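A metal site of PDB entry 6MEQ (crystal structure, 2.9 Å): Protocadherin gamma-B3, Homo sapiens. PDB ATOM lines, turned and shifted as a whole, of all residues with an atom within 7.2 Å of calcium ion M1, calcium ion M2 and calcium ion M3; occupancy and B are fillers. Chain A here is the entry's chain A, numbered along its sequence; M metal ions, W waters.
Six residues have an atom within 4 Å of calcium ion M1: Asn 206, Asn 208, Asp 238, Asp 240, Asn 244 and Asp 293.
Calcium ion M2 is bound by the side-chain carboxylate (OD1) of Asp 207 (2.4 Å), the side-chain carboxylate (OD1) of Asp 204 (2.4 Å), the side-chain carboxylate (OE2) of Glu 114 (2.4 Å), the side-chain carboxylate (OE2) of Glu 173 (2.4 Å), the side-chain carboxylate (OE1) of Glu 173 (2.6 Å) and the side-chain carboxylate (OD1) of Asp 240 (2.8 Å).
Calcium ion M2 has six donor atoms within binding distance.
Slightly farther from calcium ion M2 lies the backbone carbonyl oxygen (O) of Ala 205 (2.9 Å).
Of the 28 residues printed, 3 come within 4 Å of calcium ion M3.
The nearest printed residue that does not touch calcium ion M3 is Asn 208 (4.1 Å).
The side-chain carboxylate of Asp 293 sits close to the backbone NH of Gly 295 (3.5 Å).
OD2 of Asp 204 lies within hydrogen-bond range of ND2 of Asn 244.
OD2 of Asp 204 is in hydrogen-bond range of N of Glu 241, at 3.1 Å.
OD1 of Asp 204 sits close to NE of Arg 172 (2.6 Å).
The side-chain carboxylate (OD1) of Asp 293 lies within hydrogen-bond range of the backbone NH (N) of His 297.
The side-chain carboxylate (OE1) of Glu 114 sits at hydrogen-bond distance from the backbone NH (N) of Arg 172, 3.1 Å away.
O of Asn 206 lies within hydrogen-bond range of NE2 of His 297.
The backbone NH (N) of Glu 114 lies within hydrogen-bond range of the backbone carbonyl oxygen (O) of Ala 203.
Calcium ion M3 is bound by the side-chain carboxylate (OE1) of Glu 173 (2.5 Å).
The side-chain carboxylate (OD2) of Asp 207 binds calcium ion M3 (2.5 Å).
Water W1 binds calcium ion M3, 2.5 Å away.
OD1 of Asp 171 binds calcium ion M3 (2.5 Å).
Calcium ion M1 is bound by OD1 of Asn 206, OD2 of Asp 238, O of Asn 208, OD2 of Asp 240, OD1 of Asp 238, O of Asn 244 and OD2 of Asp 293.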
ATOM      1  N   GLU A 114       4.824 -13.523  -4.268  1.00  0.00           N
ATOM      2  CA  GLU A 114       5.138 -12.502  -3.284  1.00  0.00           C
ATOM      3  C   GLU A 114       3.951 -12.151  -2.389  1.00  0.00           C
ATOM      4  O   GLU A 114       4.153 -11.454  -1.394  1.00  0.00           O
ATOM      5  CB  GLU A 114       5.644 -11.239  -3.995  1.00  0.00           C
ATOM      6  CG  GLU A 114       4.680 -10.656  -4.997  1.00  0.00           C
ATOM      7  CD  GLU A 114       5.213  -9.400  -5.650  1.00  0.00           C
ATOM      8  OE1 GLU A 114       6.273  -8.896  -5.219  1.00  0.00           O
ATOM      9  OE2 GLU A 114       4.576  -8.914  -6.612  1.00  0.00           O
ATOM     10  N   LEU A 170       8.014 -11.397   1.073  1.00  0.00           N
ATOM     11  CA  LEU A 170       8.833 -11.348  -0.128  1.00  0.00           C
ATOM     12  C   LEU A 170       8.374 -10.222  -1.056  1.00  0.00           C
ATOM     13  O   LEU A 170       7.192  -9.875  -1.111  1.00  0.00           O
ATOM     14  CB  LEU A 170       8.769 -12.681  -0.877  1.00  0.00           C
ATOM     15  CG  LEU A 170       9.323 -13.904  -0.140  1.00  0.00           C
ATOM     16  CD1 LEU A 170       9.250 -15.136  -1.022  1.00  0.00           C
ATOM     17  CD2 LEU A 170      10.748 -13.656   0.327  1.00  0.00           C
ATOM     18  N   ASP A 171       9.335  -9.658  -1.784  1.00  0.00           N
ATOM     19  CA  ASP A 171       9.078  -8.554  -2.710  1.00  0.00           C
ATOM     20  C   ASP A 171       9.960  -8.757  -3.938  1.00  0.00           C
ATOM     21  O   ASP A 171      11.186  -8.667  -3.841  1.00  0.00           O
ATOM     22  CB  ASP A 171       9.348  -7.204  -2.054  1.00  0.00           C
ATOM     23  CG  ASP A 171       8.895  -6.032  -2.909  1.00  0.00           C
ATOM     24  OD1 ASP A 171       8.279  -6.268  -3.973  1.00  0.00           O
ATOM     25  OD2 ASP A 171       9.156  -4.871  -2.516  1.00  0.00           O
ATOM     26  N   ARG A 172       9.323  -9.032  -5.087  1.00  0.00           N
ATOM     27  CA  ARG A 172      10.095  -9.235  -6.309  1.00  0.00           C
ATOM     28  C   ARG A 172      10.736  -7.930  -6.783  1.00  0.00           C
ATOM     29  O   ARG A 172      11.811  -7.958  -7.385  1.00  0.00           O
ATOM     30  CB  ARG A 172       9.199  -9.813  -7.398  1.00  0.00           C
ATOM     31  CG  ARG A 172       9.950 -10.215  -8.662  1.00  0.00           C
ATOM     32  CD  ARG A 172       8.994 -10.406  -9.825  1.00  0.00           C
ATOM     33  NE  ARG A 172       8.264  -9.178 -10.126  1.00  0.00           N
ATOM     34  CZ  ARG A 172       8.675  -8.257 -10.996  1.00  0.00           C
ATOM     35  NH1 ARG A 172       7.938  -7.177 -11.205  1.00  0.00           N
ATOM     36  NH2 ARG A 172       9.816  -8.425 -11.655  1.00  0.00           N
ATOM     37  N   GLU A 173      10.086  -6.793  -6.526  1.00  0.00           N
ATOM     38  CA  GLU A 173      10.646  -5.508  -6.932  1.00  0.00           C
ATOM     39  C   GLU A 173      11.900  -5.149  -6.152  1.00  0.00           C
ATOM     40  O   GLU A 173      12.634  -4.243  -6.567  1.00  0.00           O
ATOM     41  CB  GLU A 173       9.597  -4.409  -6.780  1.00  0.00           C
ATOM     42  CG  GLU A 173       8.569  -4.341  -7.909  1.00  0.00           C
ATOM     43  CD  GLU A 173       7.687  -5.582  -7.987  1.00  0.00           C
ATOM     44  OE1 GLU A 173       7.505  -6.258  -6.956  1.00  0.00           O
ATOM     45  OE2 GLU A 173       7.173  -5.866  -9.086  1.00  0.00           O
ATOM     46  N   GLU A 174      12.150  -5.824  -5.032  1.00  0.00           N
ATOM     47  CA  GLU A 174      13.363  -5.603  -4.230  1.00  0.00           C
ATOM     48  C   GLU A 174      14.406  -6.694  -4.427  1.00  0.00           C
ATOM     49  O   GLU A 174      15.590  -6.392  -4.572  1.00  0.00           O
ATOM     50  CB  GLU A 174      12.992  -5.503  -2.749  1.00  0.00           C
ATOM     51  CG  GLU A 174      14.177  -5.196  -1.839  1.00  0.00           C
ATOM     52  CD  GLU A 174      14.716  -3.793  -2.019  1.00  0.00           C
ATOM     53  OE1 GLU A 174      13.981  -2.933  -2.554  1.00  0.00           O
ATOM     54  OE2 GLU A 174      15.876  -3.544  -1.629  1.00  0.00           O
ATOM     55  N   ALA A 203       7.604 -15.211  -7.572  1.00  0.00           N
ATOM     56  CA  ALA A 203       6.628 -14.956  -8.620  1.00  0.00           C
ATOM     57  C   ALA A 203       6.004 -13.575  -8.448  1.00  0.00           C
ATOM     58  O   ALA A 203       5.827 -13.090  -7.329  1.00  0.00           O
ATOM     59  CB  ALA A 203       5.532 -16.030  -8.616  1.00  0.00           C
ATOM     60  N   ASP A 204       5.665 -12.952  -9.576  1.00  0.00           N
ATOM     61  CA  ASP A 204       5.185 -11.575  -9.571  1.00  0.00           C
ATOM     62  C   ASP A 204       3.675 -11.534  -9.376  1.00  0.00           C
ATOM     63  O   ASP A 204       2.932 -12.302  -9.985  1.00  0.00           O
ATOM     64  CB  ASP A 204       5.547 -10.875 -10.878  1.00  0.00           C
ATOM     65  CG  ASP A 204       5.168  -9.405 -10.864  1.00  0.00           C
ATOM     66  OD1 ASP A 204       5.710  -8.657 -10.026  1.00  0.00           O
ATOM     67  OD2 ASP A 204       4.328  -8.993 -11.698  1.00  0.00           O
ATOM     68  N   ALA A 205       3.235 -10.623  -8.505  1.00  0.00           N
ATOM     69  CA  ALA A 205       1.825 -10.334  -8.313  1.00  0.00           C
ATOM     70  C   ALA A 205       1.605  -8.836  -8.496  1.00  0.00           C
ATOM     71  O   ALA A 205       2.521  -8.032  -8.313  1.00  0.00           O
ATOM     72  CB  ALA A 205       1.326 -10.787  -6.936  1.00  0.00           C
ATOM     73  N   ASN A 206       0.376  -8.478  -8.853  1.00  0.00           N
ATOM     74  CA  ASN A 206       0.031  -7.074  -9.131  1.00  0.00           C
ATOM     75  C   ASN A 206      -0.043  -6.316  -7.813  1.00  0.00           C
ATOM     76  O   ASN A 206      -1.112  -6.025  -7.272  1.00  0.00           O
ATOM     77  CB  ASN A 206      -1.281  -6.984  -9.907  1.00  0.00           C
ATOM     78  CG  ASN A 206      -1.380  -5.720 -10.720  1.00  0.00           C
ATOM     79  OD1 ASN A 206      -0.388  -5.220 -11.238  1.00  0.00           O
ATOM     80  ND2 ASN A 206      -2.589  -5.184 -10.831  1.00  0.00           N
ATOM     81  N   ASP A 207       1.140  -5.994  -7.273  1.00  0.00           N
ATOM     82  CA  ASP A 207       1.252  -5.270  -6.004  1.00  0.00           C
ATOM     83  C   ASP A 207       1.648  -3.812  -6.198  1.00  0.00           C
ATOM     84  O   ASP A 207       2.155  -3.181  -5.269  1.00  0.00           O
ATOM     85  CB  ASP A 207       2.247  -5.985  -5.087  1.00  0.00           C
ATOM     86  CG  ASP A 207       3.658  -6.022  -5.663  1.00  0.00           C
ATOM     87  OD1 ASP A 207       3.793  -5.910  -6.900  1.00  0.00           O
ATOM     88  OD2 ASP A 207       4.616  -6.158  -4.880  1.00  0.00           O
ATOM     89  N   ASN A 208       1.433  -3.259  -7.395  1.00  0.00           N
ATOM     90  CA  ASN A 208       1.762  -1.869  -7.662  1.00  0.00           C
ATOM     91  C   ASN A 208       0.897  -1.328  -8.796  1.00  0.00           C
ATOM     92  O   ASN A 208       1.036  -1.769  -9.942  1.00  0.00           O
ATOM     93  CB  ASN A 208       3.246  -1.728  -8.005  1.00  0.00           C
ATOM     94  CG  ASN A 208       4.012  -0.931  -6.972  1.00  0.00           C
ATOM     95  OD1 ASN A 208       3.478  -0.018  -6.344  1.00  0.00           O
ATOM     96  ND2 ASN A 208       5.279  -1.282  -6.769  1.00  0.00           N
ATOM     97  N   PRO A 209       0.016  -0.387  -8.515  1.00  0.00           N
ATOM     98  CA  PRO A 209      -0.834   0.185  -9.561  1.00  0.00           C
ATOM     99  C   PRO A 209      -0.049   1.153 -10.425  1.00  0.00           C
ATOM    100  O   PRO A 209       1.044   1.592 -10.034  1.00  0.00           O
ATOM    101  CB  PRO A 209      -1.936   0.906  -8.778  1.00  0.00           C
ATOM    102  CG  PRO A 209      -1.275   1.287  -7.498  1.00  0.00           C
ATOM    103  CD  PRO A 209      -0.297   0.178  -7.186  1.00  0.00           C
ATOM    104  N   PRO A 210      -0.557   1.500 -11.614  1.00  0.00           N
ATOM    105  CA  PRO A 210       0.143   2.480 -12.451  1.00  0.00           C
ATOM    106  C   PRO A 210       0.213   3.842 -11.783  1.00  0.00           C
ATOM    107  O   PRO A 210      -0.684   4.233 -11.017  1.00  0.00           O
ATOM    108  CB  PRO A 210      -0.709   2.527 -13.729  1.00  0.00           C
ATOM    109  CG  PRO A 210      -1.443   1.227 -13.739  1.00  0.00           C
ATOM    110  CD  PRO A 210      -1.715   0.903 -12.305  1.00  0.00           C
ATOM    111  N   ILE A 237       3.969   4.673 -15.152  1.00  0.00           N
ATOM    112  CA  ILE A 237       5.023   3.742 -14.784  1.00  0.00           C
ATOM    113  C   ILE A 237       4.425   2.638 -13.931  1.00  0.00           C
ATOM    114  O   ILE A 237       3.681   2.917 -12.978  1.00  0.00           O
ATOM    115  CB  ILE A 237       6.172   4.452 -14.043  1.00  0.00           C
ATOM    116  CG1 ILE A 237       6.733   5.591 -14.900  1.00  0.00           C
ATOM    117  CG2 ILE A 237       7.270   3.467 -13.686  1.00  0.00           C
ATOM    118  CD1 ILE A 237       7.868   6.354 -14.248  1.00  0.00           C
ATOM    119  N   ASP A 238       4.744   1.387 -14.274  1.00  0.00           N
ATOM    120  CA  ASP A 238       4.285   0.220 -13.531  1.00  0.00           C
ATOM    121  C   ASP A 238       5.502  -0.645 -13.213  1.00  0.00           C
ATOM    122  O   ASP A 238       6.228  -1.047 -14.114  1.00  0.00           O
ATOM    123  CB  ASP A 238       3.253  -0.565 -14.331  1.00  0.00           C
ATOM    124  CG  ASP A 238       2.372  -1.444 -13.452  1.00  0.00           C
ATOM    125  OD1 ASP A 238       2.870  -1.947 -12.420  1.00  0.00           O
ATOM    126  OD2 ASP A 238       1.181  -1.614 -13.784  1.00  0.00           O
ATOM    127  N   MET A 239       5.710  -0.922 -11.926  1.00  0.00           N
ATOM    128  CA  MET A 239       6.883  -1.647 -11.464  1.00  0.00           C
ATOM    129  C   MET A 239       6.721  -3.158 -11.518  1.00  0.00           C
ATOM    130  O   MET A 239       7.610  -3.880 -11.063  1.00  0.00           O
ATOM    131  CB  MET A 239       7.238  -1.219 -10.029  1.00  0.00           C
ATOM    132  CG  MET A 239       7.587   0.249  -9.886  1.00  0.00           C
ATOM    133  SD  MET A 239       9.041   0.713 -10.856  1.00  0.00           S
ATOM    134  CE  MET A 239       9.174   2.454 -10.452  1.00  0.00           C
ATOM    135  N   ASP A 240       5.616  -3.654 -12.062  1.00  0.00           N
ATOM    136  CA  ASP A 240       5.354  -5.087 -12.108  1.00  0.00           C
ATOM    137  C   ASP A 240       5.903  -5.667 -13.412  1.00  0.00           C
ATOM    138  O   ASP A 240       6.600  -4.997 -14.174  1.00  0.00           O
ATOM    139  CB  ASP A 240       3.861  -5.350 -11.931  1.00  0.00           C
ATOM    140  CG  ASP A 240       3.358  -4.944 -10.563  1.00  0.00           C
ATOM    141  OD1 ASP A 240       4.112  -5.106  -9.591  1.00  0.00           O
ATOM    142  OD2 ASP A 240       2.207  -4.466 -10.462  1.00  0.00           O
ATOM    143  N   GLU A 241       5.603  -6.945 -13.663  1.00  0.00           N
ATOM    144  CA  GLU A 241       6.167  -7.671 -14.789  1.00  0.00           C
ATOM    145  C   GLU A 241       5.077  -8.450 -15.503  1.00  0.00           C
ATOM    146  O   GLU A 241       4.201  -9.041 -14.871  1.00  0.00           O
ATOM    147  CB  GLU A 241       7.262  -8.645 -14.320  1.00  0.00           C
ATOM    148  CG  GLU A 241       7.894  -9.473 -15.430  1.00  0.00           C
ATOM    149  CD  GLU A 241       8.869 -10.514 -14.896  1.00  0.00           C
ATOM    150  OE1 GLU A 241       9.021 -10.607 -13.657  1.00  0.00           O
ATOM    151  OE2 GLU A 241       9.477 -11.234 -15.714  1.00  0.00           O
ATOM    152  N   ILE A 243       1.815  -9.281 -17.697  1.00  0.00           N
ATOM    153  CA  ILE A 243       0.497  -8.691 -17.901  1.00  0.00           C
ATOM    154  C   ILE A 243       0.212  -7.620 -16.865  1.00  0.00           C
ATOM    155  O   ILE A 243      -0.530  -6.656 -17.126  1.00  0.00           O
ATOM    156  CB  ILE A 243      -0.582  -9.802 -17.905  1.00  0.00           C
ATOM    157  CG1 ILE A 243      -1.971  -9.210 -18.150  1.00  0.00           C
ATOM    158  CG2 ILE A 243      -0.556 -10.572 -16.590  1.00  0.00           C
ATOM    159  CD1 ILE A 243      -2.118  -8.510 -19.483  1.00  0.00           C
ATOM    160  N   ASN A 244       0.789  -7.744 -15.665  1.00  0.00           N
ATOM    161  CA  ASN A 244       0.612  -6.765 -14.610  1.00  0.00           C
ATOM    162  C   ASN A 244       1.358  -5.465 -14.881  1.00  0.00           C
ATOM    163  O   ASN A 244       1.283  -4.545 -14.047  1.00  0.00           O
ATOM    164  CB  ASN A 244       1.058  -7.344 -13.271  1.00  0.00           C
ATOM    165  CG  ASN A 244       0.315  -8.617 -12.913  1.00  0.00           C
ATOM    166  OD1 ASN A 244      -0.846  -8.804 -13.299  1.00  0.00           O
ATOM    167  ND2 ASN A 244       0.975  -9.498 -12.173  1.00  0.00           N
ATOM    168  N   ALA A 245       2.069  -5.354 -15.999  1.00  0.00           N
ATOM    169  CA  ALA A 245       2.806  -4.149 -16.349  1.00  0.00           C
ATOM    170  C   ALA A 245       2.297  -3.452 -17.604  1.00  0.00           C
ATOM    171  O   ALA A 245       2.591  -2.266 -17.798  1.00  0.00           O
ATOM    172  CB  ALA A 245       4.304  -4.445 -16.527  1.00  0.00           C
ATOM    173  N   GLU A 246       1.547  -4.153 -18.462  1.00  0.00           N
ATOM    174  CA  GLU A 246       1.007  -3.522 -19.661  1.00  0.00           C
ATOM    175  C   GLU A 246      -0.070  -2.520 -19.287  1.00  0.00           C
ATOM    176  O   GLU A 246      -1.023  -2.849 -18.560  1.00  0.00           O
ATOM    177  CB  GLU A 246       0.447  -4.592 -20.601  1.00  0.00           C
ATOM    178  CG  GLU A 246       1.466  -5.640 -21.032  1.00  0.00           C
ATOM    179  CD  GLU A 246       0.859  -6.715 -21.904  1.00  0.00           C
ATOM    180  OE1 GLU A 246      -0.345  -6.628 -22.204  1.00  0.00           O
ATOM    181  OE2 GLU A 246       1.592  -7.642 -22.303  1.00  0.00           O
ATOM    182  N   ILE A 247       0.064  -1.287 -19.778  1.00  0.00           N
ATOM    183  CA  ILE A 247      -0.818  -0.185 -19.416  1.00  0.00           C
ATOM    184  C   ILE A 247      -1.574   0.264 -20.656  1.00  0.00           C
ATOM    185  O   ILE A 247      -0.975   0.407 -21.735  1.00  0.00           O
ATOM    186  CB  ILE A 247      -0.033   0.980 -18.797  1.00  0.00           C
ATOM    187  CG1 ILE A 247       0.766   0.508 -17.586  1.00  0.00           C
ATOM    188  CG2 ILE A 247      -0.983   2.108 -18.399  1.00  0.00           C
ATOM    189  CD1 ILE A 247       1.599   1.588 -16.937  1.00  0.00           C
ATOM    190  N   ASP A 293      -4.274  -1.655 -16.029  1.00  0.00           N
ATOM    191  CA  ASP A 293      -3.283  -2.703 -16.245  1.00  0.00           C
ATOM    192  C   ASP A 293      -3.946  -4.072 -16.310  1.00  0.00           C
ATOM    193  O   ASP A 293      -5.156  -4.160 -16.531  1.00  0.00           O
ATOM    194  CB  ASP A 293      -2.218  -2.678 -15.136  1.00  0.00           C
ATOM    195  CG  ASP A 293      -2.812  -2.836 -13.739  1.00  0.00           C
ATOM    196  OD1 ASP A 293      -4.058  -2.873 -13.623  1.00  0.00           O
ATOM    197  OD2 ASP A 293      -2.038  -2.927 -12.773  1.00  0.00           O
ATOM    198  N   GLY A 294      -3.160  -5.131 -16.142  1.00  0.00           N
ATOM    199  CA  GLY A 294      -3.713  -6.474 -16.200  1.00  0.00           C
ATOM    200  C   GLY A 294      -4.559  -6.831 -15.001  1.00  0.00           C
ATOM    201  O   GLY A 294      -5.558  -7.545 -15.125  1.00  0.00           O
ATOM    202  N   GLY A 295      -4.187  -6.342 -13.821  1.00  0.00           N
ATOM    203  CA  GLY A 295      -4.927  -6.633 -12.605  1.00  0.00           C
ATOM    204  C   GLY A 295      -6.031  -5.643 -12.325  1.00  0.00           C
ATOM    205  O   GLY A 295      -6.516  -5.547 -11.192  1.00  0.00           O
ATOM    206  N   HIS A 297      -5.965  -2.487 -12.018  1.00  0.00           N
ATOM    207  CA  HIS A 297      -5.608  -1.362 -11.173  1.00  0.00           C
ATOM    208  C   HIS A 297      -5.708  -0.072 -11.972  1.00  0.00           C
ATOM    209  O   HIS A 297      -5.145   0.042 -13.069  1.00  0.00           O
ATOM    210  CB  HIS A 297      -4.198  -1.532 -10.602  1.00  0.00           C
ATOM    211  CG  HIS A 297      -4.125  -2.456  -9.427  1.00  0.00           C
ATOM    212  ND1 HIS A 297      -5.230  -3.117  -8.931  1.00  0.00           N
ATOM    213  CD2 HIS A 297      -3.083  -2.816  -8.644  1.00  0.00           C
ATOM    214  CE1 HIS A 297      -4.872  -3.854  -7.895  1.00  0.00           C
ATOM    215  NE2 HIS A 297      -3.574  -3.695  -7.702  1.00  0.00           N
HETATM  216 CA    CA M   1       0.657  -3.171 -11.948  1.00  0.00          CA
HETATM  217 CA    CA M   2       5.340  -7.192  -8.159  1.00  0.00          CA
HETATM  218 CA    CA M   3       6.669  -4.773  -5.177  1.00  0.00          CA
HETATM  219  O   HOH W   1       6.379  -3.677  -2.946  1.00  0.00           O
HETATM  220  O   HOH W   2       5.388  -6.210  -2.377  1.00  0.00           O
